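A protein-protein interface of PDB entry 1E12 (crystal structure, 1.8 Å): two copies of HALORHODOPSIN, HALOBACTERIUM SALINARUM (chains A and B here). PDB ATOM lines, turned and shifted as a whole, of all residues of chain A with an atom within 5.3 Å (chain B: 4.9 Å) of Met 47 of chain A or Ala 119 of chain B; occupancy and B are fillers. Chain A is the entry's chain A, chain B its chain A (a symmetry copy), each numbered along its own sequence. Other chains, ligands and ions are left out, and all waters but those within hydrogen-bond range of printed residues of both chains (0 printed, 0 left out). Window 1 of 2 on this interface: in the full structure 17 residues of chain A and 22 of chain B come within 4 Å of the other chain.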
ATOM      1  N   TRP A  42     -32.277   2.835 -36.094  1.00  0.00           N
ATOM      2  CA  TRP A  42     -32.237   4.026 -35.247  1.00  0.00           C
ATOM      3  C   TRP A  42     -31.422   3.691 -34.008  1.00  0.00           C
ATOM      4  O   TRP A  42     -30.568   4.479 -33.601  1.00  0.00           O
ATOM      5  CB  TRP A  42     -33.652   4.467 -34.826  1.00  0.00           C
ATOM      6  CG  TRP A  42     -33.699   5.566 -33.779  1.00  0.00           C
ATOM      7  CD1 TRP A  42     -32.998   6.742 -33.778  1.00  0.00           C
ATOM      8  CD2 TRP A  42     -34.595   5.627 -32.660  1.00  0.00           C
ATOM      9  NE1 TRP A  42     -33.421   7.537 -32.735  1.00  0.00           N
ATOM     10  CE2 TRP A  42     -34.406   6.873 -32.041  1.00  0.00           C
ATOM     11  CE3 TRP A  42     -35.558   4.746 -32.135  1.00  0.00           C
ATOM     12  CZ2 TRP A  42     -35.150   7.277 -30.922  1.00  0.00           C
ATOM     13  CZ3 TRP A  42     -36.309   5.149 -31.008  1.00  0.00           C
ATOM     14  CH2 TRP A  42     -36.098   6.406 -30.426  1.00  0.00           C
ATOM     15  N   GLY A  43     -31.701   2.544 -33.392  1.00  0.00           N
ATOM     16  CA  GLY A  43     -30.919   2.187 -32.211  1.00  0.00           C
ATOM     17  C   GLY A  43     -29.410   2.188 -32.466  1.00  0.00           C
ATOM     18  O   GLY A  43     -28.663   2.746 -31.658  1.00  0.00           O
ATOM     19  N   ALA A  44     -28.955   1.578 -33.565  1.00  0.00           N
ATOM     20  CA  ALA A  44     -27.505   1.526 -33.901  1.00  0.00           C
ATOM     21  C   ALA A  44     -26.946   2.926 -34.101  1.00  0.00           C
ATOM     22  O   ALA A  44     -25.830   3.251 -33.717  1.00  0.00           O
ATOM     23  CB  ALA A  44     -27.288   0.686 -35.152  1.00  0.00           C
ATOM     24  N   THR A  45     -27.750   3.759 -34.724  1.00  0.00           N
ATOM     25  CA  THR A  45     -27.405   5.151 -34.982  1.00  0.00           C
ATOM     26  C   THR A  45     -27.209   5.931 -33.654  1.00  0.00           C
ATOM     27  O   THR A  45     -26.401   6.891 -33.552  1.00  0.00           O
ATOM     28  CB  THR A  45     -28.561   5.640 -35.899  1.00  0.00           C
ATOM     29  OG1 THR A  45     -28.048   5.862 -37.227  1.00  0.00           O
ATOM     30  CG2 THR A  45     -29.341   6.700 -35.271  1.00  0.00           C
ATOM     31  N   LEU A  46     -27.941   5.534 -32.617  1.00  0.00           N
ATOM     32  CA  LEU A  46     -27.774   6.136 -31.293  1.00  0.00           C
ATOM     33  C   LEU A  46     -26.521   5.583 -30.585  1.00  0.00           C
ATOM     34  O   LEU A  46     -25.835   6.263 -29.815  1.00  0.00           O
ATOM     35  CB  LEU A  46     -28.948   5.824 -30.375  1.00  0.00           C
ATOM     36  CG  LEU A  46     -30.236   6.557 -30.748  1.00  0.00           C
ATOM     37  CD1 LEU A  46     -31.428   5.893 -30.063  1.00  0.00           C
ATOM     38  CD2 LEU A  46     -30.094   8.012 -30.347  1.00  0.00           C
ATOM     39  N   MET A  47     -26.262   4.334 -30.826  1.00  0.00           N
ATOM     40  CA  MET A  47     -25.127   3.717 -30.165  1.00  0.00           C
ATOM     41  C   MET A  47     -23.765   4.057 -30.715  1.00  0.00           C
ATOM     42  O   MET A  47     -22.784   3.973 -29.996  1.00  0.00           O
ATOM     43  CB  MET A  47     -25.331   2.252 -30.159  1.00  0.00           C
ATOM     44  CG  MET A  47     -26.487   1.980 -29.238  1.00  0.00           C
ATOM     45  SD  MET A  47     -26.392   0.312 -28.754  1.00  0.00           S
ATOM     46  CE  MET A  47     -27.124  -0.388 -30.228  1.00  0.00           C
ATOM     47  N   ILE A  48     -23.710   4.466 -31.973  1.00  0.00           N
ATOM     48  CA  ILE A  48     -22.417   4.860 -32.529  1.00  0.00           C
ATOM     49  C   ILE A  48     -21.845   6.056 -31.725  1.00  0.00           C
ATOM     50  O   ILE A  48     -20.708   6.017 -31.249  1.00  0.00           O
ATOM     51  CB  ILE A  48     -22.586   5.143 -34.049  1.00  0.00           C
ATOM     52  CG1 ILE A  48     -22.839   3.799 -34.771  1.00  0.00           C
ATOM     53  CG2 ILE A  48     -21.314   5.842 -34.659  1.00  0.00           C
ATOM     54  CD1 ILE A  48     -23.218   4.012 -36.286  1.00  0.00           C
ATOM     55  N   PRO A  49     -22.634   7.143 -31.541  1.00  0.00           N
ATOM     56  CA  PRO A  49     -22.082   8.248 -30.761  1.00  0.00           C
ATOM     57  C   PRO A  49     -21.955   7.933 -29.252  1.00  0.00           C
ATOM     58  O   PRO A  49     -21.083   8.507 -28.598  1.00  0.00           O
ATOM     59  CB  PRO A  49     -23.023   9.426 -31.090  1.00  0.00           C
ATOM     60  CG  PRO A  49     -24.323   8.736 -31.465  1.00  0.00           C
ATOM     61  CD  PRO A  49     -23.816   7.604 -32.325  1.00  0.00           C
ATOM     62  N   LEU A  50     -22.766   7.010 -28.714  1.00  0.00           N
ATOM     63  CA  LEU A  50     -22.622   6.704 -27.312  1.00  0.00           C
ATOM     64  C   LEU A  50     -21.270   5.983 -27.116  1.00  0.00           C
ATOM     65  O   LEU A  50     -20.535   6.267 -26.124  1.00  0.00           O
ATOM     66  CB  LEU A  50     -23.739   5.790 -26.801  1.00  0.00           C
ATOM     67  CG  LEU A  50     -25.044   6.397 -26.217  1.00  0.00           C
ATOM     68  CD1 LEU A  50     -25.993   5.249 -25.738  1.00  0.00           C
ATOM     69  CD2 LEU A  50     -24.696   7.319 -24.994  1.00  0.00           C
ATOM     70  N   VAL A  51     -20.944   5.044 -28.025  1.00  0.00           N
ATOM     71  CA  VAL A  51     -19.639   4.351 -27.870  1.00  0.00           C
ATOM     72  C   VAL A  51     -18.529   5.379 -28.033  1.00  0.00           C
ATOM     73  O   VAL A  51     -17.523   5.372 -27.281  1.00  0.00           O
ATOM     74  CB  VAL A  51     -19.460   3.209 -28.902  1.00  0.00           C
ATOM     75  CG1 VAL A  51     -18.052   2.571 -28.734  1.00  0.00           C
ATOM     76  CG2 VAL A  51     -20.544   2.119 -28.687  1.00  0.00           C
ATOM     77  N   SER A  52     -18.704   6.324 -28.966  1.00  0.00           N
ATOM     78  CA  SER A  52     -17.696   7.351 -29.209  1.00  0.00           C
ATOM     79  C   SER A  52     -17.473   8.194 -27.927  1.00  0.00           C
ATOM     80  O   SER A  52     -16.317   8.410 -27.499  1.00  0.00           O
ATOM     81  CB  SER A  52     -18.145   8.206 -30.414  1.00  0.00           C
ATOM     82  OG  SER A  52     -17.196   9.202 -30.702  1.00  0.00           O
ATOM     83  N   MET A  97     -20.576  -1.595 -34.695  1.00  0.00           N
ATOM     84  CA  MET A  97     -21.889  -0.944 -34.680  1.00  0.00           C
ATOM     85  C   MET A  97     -22.153  -0.260 -36.016  1.00  0.00           C
ATOM     86  O   MET A  97     -23.279  -0.252 -36.495  1.00  0.00           O
ATOM     87  CB  MET A  97     -21.949   0.085 -33.582  1.00  0.00           C
ATOM     88  CG  MET A  97     -21.433  -0.490 -32.298  1.00  0.00           C
ATOM     89  SD  MET A  97     -22.228   0.220 -30.852  1.00  0.00           S
ATOM     90  CE  MET A  97     -23.832  -0.540 -31.458  1.00  0.00           C
ATOM     91  N   THR B 115     -28.319  -6.309 -32.107  1.00  0.00           N
ATOM     92  CA  THR B 115     -28.351  -4.903 -31.719  1.00  0.00           C
ATOM     93  C   THR B 115     -28.490  -4.786 -30.185  1.00  0.00           C
ATOM     94  O   THR B 115     -27.818  -3.988 -29.567  1.00  0.00           O
ATOM     95  CB  THR B 115     -29.528  -4.192 -32.406  1.00  0.00           C
ATOM     96  OG1 THR B 115     -29.441  -4.380 -33.834  1.00  0.00           O
ATOM     97  CG2 THR B 115     -29.492  -2.701 -32.095  1.00  0.00           C
ATOM     98  N   VAL B 116     -29.358  -5.602 -29.588  1.00  0.00           N
ATOM     99  CA  VAL B 116     -29.555  -5.551 -28.128  1.00  0.00           C
ATOM    100  C   VAL B 116     -28.329  -6.041 -27.374  1.00  0.00           C
ATOM    101  O   VAL B 116     -27.948  -5.453 -26.354  1.00  0.00           O
ATOM    102  CB  VAL B 116     -30.830  -6.355 -27.720  1.00  0.00           C
ATOM    103  CG1 VAL B 116     -30.943  -6.435 -26.199  1.00  0.00           C
ATOM    104  CG2 VAL B 116     -32.079  -5.665 -28.332  1.00  0.00           C
ATOM    105  N   ILE B 117     -27.684  -7.114 -27.848  1.00  0.00           N
ATOM    106  CA  ILE B 117     -26.464  -7.589 -27.172  1.00  0.00           C
ATOM    107  C   ILE B 117     -25.359  -6.563 -27.296  1.00  0.00           C
ATOM    108  O   ILE B 117     -24.571  -6.374 -26.365  1.00  0.00           O
ATOM    109  CB  ILE B 117     -25.971  -8.948 -27.731  1.00  0.00           C
ATOM    110  CG1 ILE B 117     -26.930 -10.027 -27.218  1.00  0.00           C
ATOM    111  CG2 ILE B 117     -24.487  -9.239 -27.290  1.00  0.00           C
ATOM    112  CD1 ILE B 117     -26.903 -11.320 -28.020  1.00  0.00           C
ATOM    113  N   ALA B 118     -25.316  -5.879 -28.445  1.00  0.00           N
ATOM    114  CA  ALA B 118     -24.293  -4.816 -28.612  1.00  0.00           C
ATOM    115  C   ALA B 118     -24.536  -3.714 -27.558  1.00  0.00           C
ATOM    116  O   ALA B 118     -23.612  -3.254 -26.899  1.00  0.00           O
ATOM    117  CB  ALA B 118     -24.378  -4.194 -30.012  1.00  0.00           C
ATOM    118  N   ALA B 119     -25.784  -3.295 -27.412  1.00  0.00           N
ATOM    119  CA  ALA B 119     -26.045  -2.251 -26.426  1.00  0.00           C
ATOM    120  C   ALA B 119     -25.698  -2.768 -25.031  1.00  0.00           C
ATOM    121  O   ALA B 119     -25.189  -2.039 -24.199  1.00  0.00           O
ATOM    122  CB  ALA B 119     -27.503  -1.830 -26.457  1.00  0.00           C
ATOM    123  N   ASP B 120     -26.044  -4.020 -24.773  1.00  0.00           N
ATOM    124  CA  ASP B 120     -25.783  -4.617 -23.472  1.00  0.00           C
ATOM    125  C   ASP B 120     -24.292  -4.675 -23.157  1.00  0.00           C
ATOM    126  O   ASP B 120     -23.847  -4.411 -22.023  1.00  0.00           O
ATOM    127  CB  ASP B 120     -26.423  -6.020 -23.375  1.00  0.00           C
ATOM    128  CG  ASP B 120     -26.120  -6.655 -22.051  1.00  0.00           C
ATOM    129  OD1 ASP B 120     -26.902  -6.410 -21.118  1.00  0.00           O
ATOM    130  OD2 ASP B 120     -25.066  -7.326 -21.915  1.00  0.00           O
ATOM    131  N   ILE B 121     -23.490  -5.003 -24.168  1.00  0.00           N
ATOM    132  CA  ILE B 121     -22.047  -5.031 -23.915  1.00  0.00           C
ATOM    133  C   ILE B 121     -21.561  -3.595 -23.623  1.00  0.00           C
ATOM    134  O   ILE B 121     -20.702  -3.398 -22.788  1.00  0.00           O
ATOM    135  CB  ILE B 121     -21.293  -5.647 -25.137  1.00  0.00           C
ATOM    136  CG1 ILE B 121     -21.439  -7.185 -25.102  1.00  0.00           C
ATOM    137  CG2 ILE B 121     -19.747  -5.296 -25.093  1.00  0.00           C
ATOM    138  CD1 ILE B 121     -21.290  -7.876 -26.534  1.00  0.00           C
ATOM    139  N   GLY B 122     -22.125  -2.612 -24.328  1.00  0.00           N
ATOM    140  CA  GLY B 122     -21.723  -1.208 -24.123  1.00  0.00           C
ATOM    141  C   GLY B 122     -22.033  -0.840 -22.678  1.00  0.00           C
ATOM    142  O   GLY B 122     -21.266  -0.186 -22.009  1.00  0.00           O
ATOM    143  N   MET B 123     -23.199  -1.292 -22.204  1.00  0.00           N
ATOM    144  CA  MET B 123     -23.579  -1.036 -20.834  1.00  0.00           C
ATOM    145  C   MET B 123     -22.570  -1.588 -19.822  1.00  0.00           C
ATOM    146  O   MET B 123     -22.216  -0.948 -18.803  1.00  0.00           O
ATOM    147  CB  MET B 123     -24.969  -1.672 -20.556  1.00  0.00           C
ATOM    148  CG  MET B 123     -25.387  -1.515 -19.071  1.00  0.00           C
ATOM    149  SD  MET B 123     -27.015  -2.379 -18.694  1.00  0.00           S
ATOM    150  CE  MET B 123     -26.414  -4.032 -18.585  1.00  0.00           C
ATOM    151  N   PHE B 150     -27.044   3.068 -22.372  1.00  0.00           N
ATOM    152  CA  PHE B 150     -27.059   1.777 -23.041  1.00  0.00           C
ATOM    153  C   PHE B 150     -28.150   0.871 -22.427  1.00  0.00           C
ATOM    154  O   PHE B 150     -28.830   0.136 -23.131  1.00  0.00           O
ATOM    155  CB  PHE B 150     -25.706   1.093 -22.887  1.00  0.00           C
ATOM    156  CG  PHE B 150     -24.669   1.627 -23.830  1.00  0.00           C
ATOM    157  CD1 PHE B 150     -24.787   1.363 -25.203  1.00  0.00           C
ATOM    158  CD2 PHE B 150     -23.557   2.290 -23.343  1.00  0.00           C
ATOM    159  CE1 PHE B 150     -23.805   1.748 -26.099  1.00  0.00           C
ATOM    160  CE2 PHE B 150     -22.538   2.699 -24.212  1.00  0.00           C
ATOM    161  CZ  PHE B 150     -22.680   2.413 -25.619  1.00  0.00           C
ATOM    162  N   VAL B 153     -31.492   1.360 -23.961  1.00  0.00           N
ATOM    163  CA  VAL B 153     -31.691   0.717 -25.238  1.00  0.00           C
ATOM    164  C   VAL B 153     -32.109  -0.734 -25.018  1.00  0.00           C
ATOM    165  O   VAL B 153     -33.034  -1.231 -25.688  1.00  0.00           O
ATOM    166  CB  VAL B 153     -30.404   0.793 -26.099  1.00  0.00           C
ATOM    167  CG1 VAL B 153     -30.564  -0.068 -27.350  1.00  0.00           C
ATOM    168  CG2 VAL B 153     -30.129   2.276 -26.475  1.00  0.00           C
ATOM    169  N   VAL B 154     -31.463  -1.410 -24.066  1.00  0.00           N
ATOM    170  CA  VAL B 154     -31.822  -2.801 -23.793  1.00  0.00           C
ATOM    171  C   VAL B 154     -33.254  -2.874 -23.262  1.00  0.00           C
ATOM    172  O   VAL B 154     -34.068  -3.693 -23.730  1.00  0.00           O
ATOM    173  CB  VAL B 154     -30.885  -3.437 -22.737  1.00  0.00           C
ATOM    174  CG1 VAL B 154     -31.404  -4.833 -22.323  1.00  0.00           C
ATOM    175  CG2 VAL B 154     -29.436  -3.502 -23.307  1.00  0.00           C
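No position is printed for both chains. Of the 6 pairs that touch across the chains among the printed residues, none has its exchanged pair printed and touching as well.
Met 47 of chain A touches three residues of chain B. Ile 48 of chain A touches none of the printed residues of chain B. Ser 52 of chain A touches none of the printed residues of chain B. Of the printed residues of chain B, Met 97 of chain A touches Ala 118. Of the printed residues of chain A, Thr 115 of chain B touches Met 47. Of the printed residues of chain A, Ala 118 of chain B touches Met 97. Ala 119 of chain B touches just one residue of chain A: Met 47. Printed residues of chain A within 4 Å of Phe 150 of chain B: Met 47 (3.98 Å), Leu 50 (3.7 Å) and Val 51 (3.7 Å). The nearest residue of chain B that does not touch Met 47 of chain A is Val 153 of chain B (4.4 Å). The nearest printed residue of chain A that does not touch Ala 119 of chain B is Met 97 of chain A (5.3 Å).
Of the 12 printed residues of chain B, 4 touch a printed residue of chain A. Of the 12 printed residues of chain A, 4 touch a printed residue of chain B. Printed residues of chain A that touch a printed residue of chain B: Met 47, Leu 50, Val 51 and Met 97. Hydrophobic or aromatic side chains of chain A within 4 Å of the printed part of chain B: Met 47, Leu 50, Val 51 and Met 97. Among the printed residues, 6 pairs touch across the chains.
Met 47 of chain A touches Thr 115 of chain B. SD of Met 47 of chain A touches CB of Ala 119 of chain B, at 3.3 Å. Met 47 of chain A touches Phe 150 of chain B. Phe 150 of chain B touches Leu 50 of chain A (CZ to CB, 3.7 Å). Val 51 of chain A touches Phe 150 of chain B. CE of Met 97 of chain A touches CB of Ala 118 of chain B, 3.97 Å away.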
